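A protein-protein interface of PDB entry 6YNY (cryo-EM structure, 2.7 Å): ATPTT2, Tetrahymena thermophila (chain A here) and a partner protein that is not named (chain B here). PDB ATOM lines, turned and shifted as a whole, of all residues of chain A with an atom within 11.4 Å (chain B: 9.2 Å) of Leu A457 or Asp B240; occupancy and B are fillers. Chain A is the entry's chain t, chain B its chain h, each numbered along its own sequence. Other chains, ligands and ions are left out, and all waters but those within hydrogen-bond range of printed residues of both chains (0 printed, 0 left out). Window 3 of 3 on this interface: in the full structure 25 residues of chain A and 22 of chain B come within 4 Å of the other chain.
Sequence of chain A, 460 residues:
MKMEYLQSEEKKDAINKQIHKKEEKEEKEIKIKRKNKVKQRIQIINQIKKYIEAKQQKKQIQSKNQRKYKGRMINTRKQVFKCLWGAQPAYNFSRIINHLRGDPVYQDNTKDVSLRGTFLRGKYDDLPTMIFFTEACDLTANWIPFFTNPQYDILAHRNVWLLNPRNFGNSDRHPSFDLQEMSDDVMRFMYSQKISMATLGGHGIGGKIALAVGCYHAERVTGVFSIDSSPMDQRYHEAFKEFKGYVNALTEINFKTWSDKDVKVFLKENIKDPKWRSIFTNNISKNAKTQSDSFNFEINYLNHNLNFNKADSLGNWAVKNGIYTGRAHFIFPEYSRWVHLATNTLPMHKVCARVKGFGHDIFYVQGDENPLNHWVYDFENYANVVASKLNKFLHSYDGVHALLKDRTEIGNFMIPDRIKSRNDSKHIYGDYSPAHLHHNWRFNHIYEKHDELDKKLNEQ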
ATOM      1  N   ILE A 446     -21.533   7.041 -13.774  1.00  0.00           N
ATOM      2  CA  ILE A 446     -21.678   8.484 -13.627  1.00  0.00           C
ATOM      3  C   ILE A 446     -22.425   8.816 -12.344  1.00  0.00           C
ATOM      4  O   ILE A 446     -22.138   9.821 -11.681  1.00  0.00           O
ATOM      5  CB  ILE A 446     -22.379   9.074 -14.863  1.00  0.00           C
ATOM      6  CG1 ILE A 446     -22.341  10.597 -14.815  1.00  0.00           C
ATOM      7  CG2 ILE A 446     -23.808   8.585 -14.942  1.00  0.00           C
ATOM      8  CD1 ILE A 446     -22.793  11.244 -16.085  1.00  0.00           C
ATOM      9  N   GLU A 448     -22.467   6.915  -9.533  1.00  0.00           N
ATOM     10  CA  GLU A 448     -21.553   6.655  -8.427  1.00  0.00           C
ATOM     11  C   GLU A 448     -20.507   7.755  -8.311  1.00  0.00           C
ATOM     12  O   GLU A 448     -20.104   8.125  -7.203  1.00  0.00           O
ATOM     13  CB  GLU A 448     -20.885   5.297  -8.613  1.00  0.00           C
ATOM     14  CG  GLU A 448     -21.861   4.143  -8.729  1.00  0.00           C
ATOM     15  CD  GLU A 448     -21.167   2.800  -8.833  1.00  0.00           C
ATOM     16  OE1 GLU A 448     -19.924   2.761  -8.723  1.00  0.00           O
ATOM     17  OE2 GLU A 448     -21.866   1.783  -9.026  1.00  0.00           O
ATOM     18  N   LYS A 449     -20.057   8.294  -9.446  1.00  0.00           N
ATOM     19  CA  LYS A 449     -19.047   9.345  -9.417  1.00  0.00           C
ATOM     20  C   LYS A 449     -19.619  10.649  -8.881  1.00  0.00           C
ATOM     21  O   LYS A 449     -19.012  11.297  -8.020  1.00  0.00           O
ATOM     22  CB  LYS A 449     -18.481   9.562 -10.818  1.00  0.00           C
ATOM     23  CG  LYS A 449     -17.639   8.422 -11.341  1.00  0.00           C
ATOM     24  CD  LYS A 449     -17.230   8.675 -12.778  1.00  0.00           C
ATOM     25  CE  LYS A 449     -16.398   7.539 -13.332  1.00  0.00           C
ATOM     26  NZ  LYS A 449     -15.954   7.825 -14.721  1.00  0.00           N
ATOM     27  N   HIS A 450     -20.786  11.055  -9.380  1.00  0.00           N
ATOM     28  CA  HIS A 450     -21.354  12.331  -8.960  1.00  0.00           C
ATOM     29  C   HIS A 450     -21.804  12.292  -7.508  1.00  0.00           C
ATOM     30  O   HIS A 450     -21.807  13.328  -6.835  1.00  0.00           O
ATOM     31  CB  HIS A 450     -22.515  12.710  -9.874  1.00  0.00           C
ATOM     32  CG  HIS A 450     -22.094  13.063 -11.266  1.00  0.00           C
ATOM     33  ND1 HIS A 450     -22.747  14.009 -12.024  1.00  0.00           N
ATOM     34  CD2 HIS A 450     -21.087  12.592 -12.038  1.00  0.00           C
ATOM     35  CE1 HIS A 450     -22.158  14.108 -13.202  1.00  0.00           C
ATOM     36  NE2 HIS A 450     -21.148  13.259 -13.236  1.00  0.00           N
ATOM     37  N   ASP A 451     -22.188  11.117  -7.010  1.00  0.00           N
ATOM     38  CA  ASP A 451     -22.522  10.993  -5.596  1.00  0.00           C
ATOM     39  C   ASP A 451     -21.333  11.363  -4.720  1.00  0.00           C
ATOM     40  O   ASP A 451     -21.494  12.024  -3.687  1.00  0.00           O
ATOM     41  CB  ASP A 451     -22.990   9.572  -5.292  1.00  0.00           C
ATOM     42  CG  ASP A 451     -24.332   9.255  -5.913  1.00  0.00           C
ATOM     43  OD1 ASP A 451     -24.919  10.152  -6.552  1.00  0.00           O
ATOM     44  OD2 ASP A 451     -24.800   8.108  -5.764  1.00  0.00           O
ATOM     45  N   GLU A 452     -20.129  10.947  -5.115  1.00  0.00           N
ATOM     46  CA  GLU A 452     -18.934  11.302  -4.360  1.00  0.00           C
ATOM     47  C   GLU A 452     -18.683  12.803  -4.406  1.00  0.00           C
ATOM     48  O   GLU A 452     -18.417  13.431  -3.375  1.00  0.00           O
ATOM     49  CB  GLU A 452     -17.728  10.544  -4.910  1.00  0.00           C
ATOM     50  CG  GLU A 452     -17.870   9.040  -4.862  1.00  0.00           C
ATOM     51  CD  GLU A 452     -16.708   8.326  -5.519  1.00  0.00           C
ATOM     52  OE1 GLU A 452     -15.775   9.013  -5.984  1.00  0.00           O
ATOM     53  OE2 GLU A 452     -16.727   7.079  -5.574  1.00  0.00           O
ATOM     54  N   LEU A 453     -18.765  13.395  -5.597  1.00  0.00           N
ATOM     55  CA  LEU A 453     -18.558  14.832  -5.723  1.00  0.00           C
ATOM     56  C   LEU A 453     -19.573  15.612  -4.904  1.00  0.00           C
ATOM     57  O   LEU A 453     -19.249  16.673  -4.358  1.00  0.00           O
ATOM     58  CB  LEU A 453     -18.634  15.238  -7.192  1.00  0.00           C
ATOM     59  CG  LEU A 453     -17.584  14.595  -8.096  1.00  0.00           C
ATOM     60  CD1 LEU A 453     -17.963  14.752  -9.550  1.00  0.00           C
ATOM     61  CD2 LEU A 453     -16.224  15.208  -7.836  1.00  0.00           C
ATOM     62  N   ASP A 454     -20.803  15.108  -4.805  1.00  0.00           N
ATOM     63  CA  ASP A 454     -21.820  15.791  -4.015  1.00  0.00           C
ATOM     64  C   ASP A 454     -21.447  15.802  -2.538  1.00  0.00           C
ATOM     65  O   ASP A 454     -21.684  16.796  -1.840  1.00  0.00           O
ATOM     66  CB  ASP A 454     -23.177  15.121  -4.229  1.00  0.00           C
ATOM     67  CG  ASP A 454     -24.332  15.952  -3.703  1.00  0.00           C
ATOM     68  OD1 ASP A 454     -24.161  16.646  -2.679  1.00  0.00           O
ATOM     69  OD2 ASP A 454     -25.418  15.912  -4.320  1.00  0.00           O
ATOM     70  N   LYS A 455     -20.860  14.711  -2.043  1.00  0.00           N
ATOM     71  CA  LYS A 455     -20.454  14.665  -0.643  1.00  0.00           C
ATOM     72  C   LYS A 455     -19.346  15.670  -0.358  1.00  0.00           C
ATOM     73  O   LYS A 455     -19.324  16.293   0.710  1.00  0.00           O
ATOM     74  CB  LYS A 455     -19.997  13.256  -0.274  1.00  0.00           C
ATOM     75  CG  LYS A 455     -21.116  12.236  -0.224  1.00  0.00           C
ATOM     76  CD  LYS A 455     -20.603  10.881   0.222  1.00  0.00           C
ATOM     77  CE  LYS A 455     -21.737   9.884   0.391  1.00  0.00           C
ATOM     78  NZ  LYS A 455     -21.254   8.565   0.881  1.00  0.00           N
ATOM     79  N   LYS A 456     -18.418  15.840  -1.301  1.00  0.00           N
ATOM     80  CA  LYS A 456     -17.326  16.784  -1.098  1.00  0.00           C
ATOM     81  C   LYS A 456     -17.850  18.197  -0.899  1.00  0.00           C
ATOM     82  O   LYS A 456     -17.269  18.975  -0.133  1.00  0.00           O
ATOM     83  CB  LYS A 456     -16.368  16.727  -2.284  1.00  0.00           C
ATOM     84  CG  LYS A 456     -15.735  15.362  -2.482  1.00  0.00           C
ATOM     85  CD  LYS A 456     -14.966  15.281  -3.786  1.00  0.00           C
ATOM     86  CE  LYS A 456     -14.483  13.866  -4.042  1.00  0.00           C
ATOM     87  NZ  LYS A 456     -13.863  13.719  -5.385  1.00  0.00           N
ATOM     88  N   LEU A 457     -18.943  18.546  -1.576  1.00  0.00           N
ATOM     89  CA  LEU A 457     -19.566  19.847  -1.368  1.00  0.00           C
ATOM     90  C   LEU A 457     -20.034  19.996   0.073  1.00  0.00           C
ATOM     91  O   LEU A 457     -19.808  21.032   0.711  1.00  0.00           O
ATOM     92  CB  LEU A 457     -20.740  20.014  -2.331  1.00  0.00           C
ATOM     93  CG  LEU A 457     -20.374  20.190  -3.803  1.00  0.00           C
ATOM     94  CD1 LEU A 457     -21.608  20.058  -4.675  1.00  0.00           C
ATOM     95  CD2 LEU A 457     -19.701  21.528  -4.030  1.00  0.00           C
ATOM     96  N   ASN A 458     -20.688  18.969   0.601  1.00  0.00           N
ATOM     97  CA  ASN A 458     -21.204  18.994   1.962  1.00  0.00           C
ATOM     98  C   ASN A 458     -20.163  18.477   2.948  1.00  0.00           C
ATOM     99  O   ASN A 458     -19.068  19.027   3.054  1.00  0.00           O
ATOM    100  CB  ASN A 458     -22.478  18.157   2.054  1.00  0.00           C
ATOM    101  CG  ASN A 458     -23.546  18.615   1.083  1.00  0.00           C
ATOM    102  OD1 ASN A 458     -23.813  19.809   0.954  1.00  0.00           O
ATOM    103  ND2 ASN A 458     -24.154  17.665   0.383  1.00  0.00           N
ATOM    104  N   ARG B 236     -28.947  26.138 -13.608  1.00  0.00           N
ATOM    105  CA  ARG B 236     -28.198  25.165 -12.816  1.00  0.00           C
ATOM    106  C   ARG B 236     -26.736  25.584 -12.802  1.00  0.00           C
ATOM    107  O   ARG B 236     -25.956  25.189 -13.679  1.00  0.00           O
ATOM    108  CB  ARG B 236     -28.367  23.760 -13.381  1.00  0.00           C
ATOM    109  CG  ARG B 236     -29.802  23.304 -13.411  1.00  0.00           C
ATOM    110  CD  ARG B 236     -29.972  21.989 -14.123  1.00  0.00           C
ATOM    111  NE  ARG B 236     -31.284  21.899 -14.752  1.00  0.00           N
ATOM    112  CZ  ARG B 236     -31.552  22.321 -15.983  1.00  0.00           C
ATOM    113  NH1 ARG B 236     -30.601  22.860 -16.734  1.00  0.00           N
ATOM    114  NH2 ARG B 236     -32.777  22.202 -16.468  1.00  0.00           N
ATOM    115  N   PRO B 237     -26.323  26.380 -11.817  1.00  0.00           N
ATOM    116  CA  PRO B 237     -24.949  26.888 -11.802  1.00  0.00           C
ATOM    117  C   PRO B 237     -23.926  25.771 -11.674  1.00  0.00           C
ATOM    118  O   PRO B 237     -24.242  24.610 -11.409  1.00  0.00           O
ATOM    119  CB  PRO B 237     -24.926  27.815 -10.584  1.00  0.00           C
ATOM    120  CG  PRO B 237     -26.340  28.175 -10.354  1.00  0.00           C
ATOM    121  CD  PRO B 237     -27.140  26.990 -10.759  1.00  0.00           C
ATOM    122  N   ALA B 238     -22.667  26.149 -11.873  1.00  0.00           N
ATOM    123  CA  ALA B 238     -21.548  25.215 -11.841  1.00  0.00           C
ATOM    124  C   ALA B 238     -21.031  25.113 -10.412  1.00  0.00           C
ATOM    125  O   ALA B 238     -20.454  26.068  -9.884  1.00  0.00           O
ATOM    126  CB  ALA B 238     -20.447  25.670 -12.792  1.00  0.00           C
ATOM    127  N   GLN B 239     -21.242  23.956  -9.787  1.00  0.00           N
ATOM    128  CA  GLN B 239     -20.753  23.736  -8.432  1.00  0.00           C
ATOM    129  C   GLN B 239     -19.291  23.311  -8.424  1.00  0.00           C
ATOM    130  O   GLN B 239     -18.475  23.875  -7.686  1.00  0.00           O
ATOM    131  CB  GLN B 239     -21.604  22.674  -7.742  1.00  0.00           C
ATOM    132  CG  GLN B 239     -22.977  23.139  -7.324  1.00  0.00           C
ATOM    133  CD  GLN B 239     -23.892  21.983  -6.985  1.00  0.00           C
ATOM    134  OE1 GLN B 239     -23.913  20.969  -7.681  1.00  0.00           O
ATOM    135  NE2 GLN B 239     -24.645  22.123  -5.903  1.00  0.00           N
ATOM    136  N   ASP B 240     -18.944  22.319  -9.242  1.00  0.00           N
ATOM    137  CA  ASP B 240     -17.619  21.715  -9.211  1.00  0.00           C
ATOM    138  C   ASP B 240     -16.964  21.736 -10.584  1.00  0.00           C
ATOM    139  O   ASP B 240     -17.452  22.393 -11.509  1.00  0.00           O
ATOM    140  CB  ASP B 240     -17.713  20.276  -8.699  1.00  0.00           C
ATOM    141  CG  ASP B 240     -18.250  20.196  -7.288  1.00  0.00           C
ATOM    142  OD1 ASP B 240     -18.371  21.254  -6.639  1.00  0.00           O
ATOM    143  OD2 ASP B 240     -18.554  19.074  -6.830  1.00  0.00           O
ATOM    144  N   VAL B 241     -15.846  21.017 -10.719  1.00  0.00           N
ATOM    145  CA  VAL B 241     -15.146  20.927 -11.994  1.00  0.00           C
ATOM    146  C   VAL B 241     -16.050  20.411 -13.101  1.00  0.00           C
ATOM    147  O   VAL B 241     -15.758  20.619 -14.283  1.00  0.00           O
ATOM    148  CB  VAL B 241     -13.908  20.020 -11.846  1.00  0.00           C
ATOM    149  CG1 VAL B 241     -13.174  19.910 -13.165  1.00  0.00           C
ATOM    150  CG2 VAL B 241     -12.987  20.549 -10.764  1.00  0.00           C
ATOM    151  N   ARG B 242     -17.145  19.736 -12.747  1.00  0.00           N
ATOM    152  CA  ARG B 242     -18.076  19.252 -13.759  1.00  0.00           C
ATOM    153  C   ARG B 242     -18.522  20.372 -14.686  1.00  0.00           C
ATOM    154  O   ARG B 242     -18.680  20.165 -15.894  1.00  0.00           O
ATOM    155  CB  ARG B 242     -19.280  18.607 -13.078  1.00  0.00           C
ATOM    156  CG  ARG B 242     -18.944  17.325 -12.359  1.00  0.00           C
ATOM    157  CD  ARG B 242     -20.107  16.817 -11.542  1.00  0.00           C
ATOM    158  NE  ARG B 242     -20.267  17.554 -10.296  1.00  0.00           N
ATOM    159  CZ  ARG B 242     -21.133  17.229  -9.345  1.00  0.00           C
ATOM    160  NH1 ARG B 242     -21.920  16.175  -9.494  1.00  0.00           N
ATOM    161  NH2 ARG B 242     -21.211  17.954  -8.241  1.00  0.00           N
ATOM    162  N   GLY B 243     -18.735  21.564 -14.138  1.00  0.00           N
ATOM    163  CA  GLY B 243     -19.088  22.713 -14.931  1.00  0.00           C
ATOM    164  C   GLY B 243     -20.551  23.069 -14.797  1.00  0.00           C
ATOM    165  O   GLY B 243     -21.277  22.516 -13.967  1.00  0.00           O
ATOM    166  N   PRO B 244     -21.011  24.016 -15.612  1.00  0.00           N
ATOM    167  CA  PRO B 244     -22.424  24.404 -15.561  1.00  0.00           C
ATOM    168  C   PRO B 244     -23.320  23.258 -16.005  1.00  0.00           C
ATOM    169  O   PRO B 244     -23.104  22.654 -17.057  1.00  0.00           O
ATOM    170  CB  PRO B 244     -22.504  25.590 -16.528  1.00  0.00           C
ATOM    171  CG  PRO B 244     -21.103  26.049 -16.708  1.00  0.00           C
ATOM    172  CD  PRO B 244     -20.252  24.839 -16.565  1.00  0.00           C
ATOM    173  N   ASP B 245     -24.336  22.966 -15.196  1.00  0.00           N
ATOM    174  CA  ASP B 245     -25.310  21.926 -15.513  1.00  0.00           C
ATOM    175  C   ASP B 245     -24.611  20.606 -15.826  1.00  0.00           C
ATOM    176  O   ASP B 245     -24.844  19.977 -16.860  1.00  0.00           O
ATOM    177  CB  ASP B 245     -26.201  22.364 -16.672  1.00  0.00           C
ATOM    178  CG  ASP B 245     -27.382  21.444 -16.877  1.00  0.00           C
ATOM    179  OD1 ASP B 245     -27.502  20.444 -16.140  1.00  0.00           O
ATOM    180  OD2 ASP B 245     -28.198  21.726 -17.773  1.00  0.00           O
ATOM    181  N   GLY B 246     -23.736  20.187 -14.917  1.00  0.00           N
ATOM    182  CA  GLY B 246     -22.999  18.954 -15.097  1.00  0.00           C
ATOM    183  C   GLY B 246     -23.318  17.868 -14.092  1.00  0.00           C
ATOM    184  O   GLY B 246     -22.557  16.905 -13.968  1.00  0.00           O
ATOM    185  N   ASN B 247     -24.424  18.003 -13.366  1.00  0.00           N
ATOM    186  CA  ASN B 247     -24.820  17.035 -12.352  1.00  0.00           C
ATOM    187  C   ASN B 247     -26.041  16.261 -12.825  1.00  0.00           C
ATOM    188  O   ASN B 247     -27.059  16.859 -13.187  1.00  0.00           O
ATOM    189  CB  ASN B 247     -25.124  17.731 -11.028  1.00  0.00           C
ATOM    190  CG  ASN B 247     -25.283  16.759  -9.885  1.00  0.00           C
ATOM    191  OD1 ASN B 247     -25.603  15.590 -10.085  1.00  0.00           O
ATOM    192  ND2 ASN B 247     -25.060  17.240  -8.673  1.00  0.00           N
ATOM    193  N   ASN B 249     -27.684  14.206 -10.826  1.00  0.00           N
ATOM    194  CA  ASN B 249     -28.610  14.093  -9.708  1.00  0.00           C
ATOM    195  C   ASN B 249     -29.670  15.182  -9.728  1.00  0.00           C
ATOM    196  O   ASN B 249     -30.751  14.990  -9.163  1.00  0.00           O
ATOM    197  CB  ASN B 249     -27.835  14.125  -8.395  1.00  0.00           C
ATOM    198  CG  ASN B 249     -26.839  12.994  -8.281  1.00  0.00           C
ATOM    199  OD1 ASN B 249     -27.071  11.893  -8.778  1.00  0.00           O
ATOM    200  ND2 ASN B 249     -25.719  13.258  -7.628  1.00  0.00           N
ATOM    201  N   ASP B 250     -29.387  16.319 -10.364  1.00  0.00           N
ATOM    202  CA  ASP B 250     -30.376  17.386 -10.448  1.00  0.00           C
ATOM    203  C   ASP B 250     -31.608  16.945 -11.225  1.00  0.00           C
ATOM    204  O   ASP B 250     -32.699  17.485 -11.016  1.00  0.00           O
ATOM    205  CB  ASP B 250     -29.761  18.621 -11.099  1.00  0.00           C
ATOM    206  CG  ASP B 250     -28.636  19.210 -10.282  1.00  0.00           C
ATOM    207  OD1 ASP B 250     -28.615  18.989  -9.053  1.00  0.00           O
ATOM    208  OD2 ASP B 250     -27.774  19.898 -10.866  1.00  0.00           O
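ND1 of His A450 sits at hydrogen-bond distance from NH1 of Arg B242 (3.4 Å).
ND1 of His A450 sits close to O of Gly B246 (3.5 Å).
The side-chain amide nitrogen (ND2) of Asn B249 sits at hydrogen-bond distance from the side-chain carboxylate (OD1) of Asp A451 (3.4 Å).
The side-chain carboxylate of Asp B240 is in salt-bridge range of the guanidinium group of Arg B242 (3.2 Å).
NH1 of Arg B242 sits close to ND2 of Asn B247.
The backbone NH (N) of Asn B249 lies within hydrogen-bond range of the side-chain amide oxygen (OD1) of Asn B247 (2.6 Å).
Among the printed residues, merely in contact across the chains: Leu A457 with Asp B240 (2.9 Å), Leu A453 with Asp B240 (3.5 Å), Leu A453 with Arg B242 (3.6 Å), His A450 with Asn B247 (3.7 Å), Leu A457 with Gln B239 (3.8 Å) and His A450 with Asn B249 (3.95 Å).
Of the printed residues of chain B, His A450 touches Arg B242 (3.4 Å), Gly B246 (2.9 Å), Asn B247 (3.7 Å) and Asn B249 (3.95 Å).
Printed residues of chain B within 4 Å of Asp A451: Asn B249 (3.4 Å).
Printed residues of chain B within 4 Å of Leu A453: Asp B240 (3.5 Å) and Arg B242 (3.6 Å).
Asp A454 touches none of the printed residues of chain B.
Leu A457 touches just these residues of chain B: Gln B239 (3.8 Å) and Asp B240 (2.9 Å).
No residue of chain B comes within 4 Å of Asn A458.
Gln B239 touches just one residue of chain A: Leu A457 (3.8 Å).
Of chain A, only Leu A453 and Leu A457 come within 4 Å of Asp B240.
No residue of chain A comes within 4 Å of Val B241.
Arg B242 touches two residues of chain A.
No residue of chain A comes within 4 Å of Gly B243.
Pro B244 touches none of the printed residues of chain A.
Of the printed residues of chain A, Gly B246 touches His A450 (2.9 Å).
The nearest residue of chain B that does not touch Leu A457 is Arg B242 (4.2 Å).
The nearest residue of chain A that does not touch Asp B240 is Asp A454 (5.0 Å).
The nearest printed residue of chain A that does not touch Asn B249 is Asp A454 (4.3 Å).
Hydrophobic or aromatic side chains of chain A within 4 Å of the printed part of chain B: His A450, Leu A453 and Leu A457.
Among the printed residues, no Asp or Glu carboxylate lies within 4 Å of a Lys or Arg side-chain nitrogen of the other chain.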
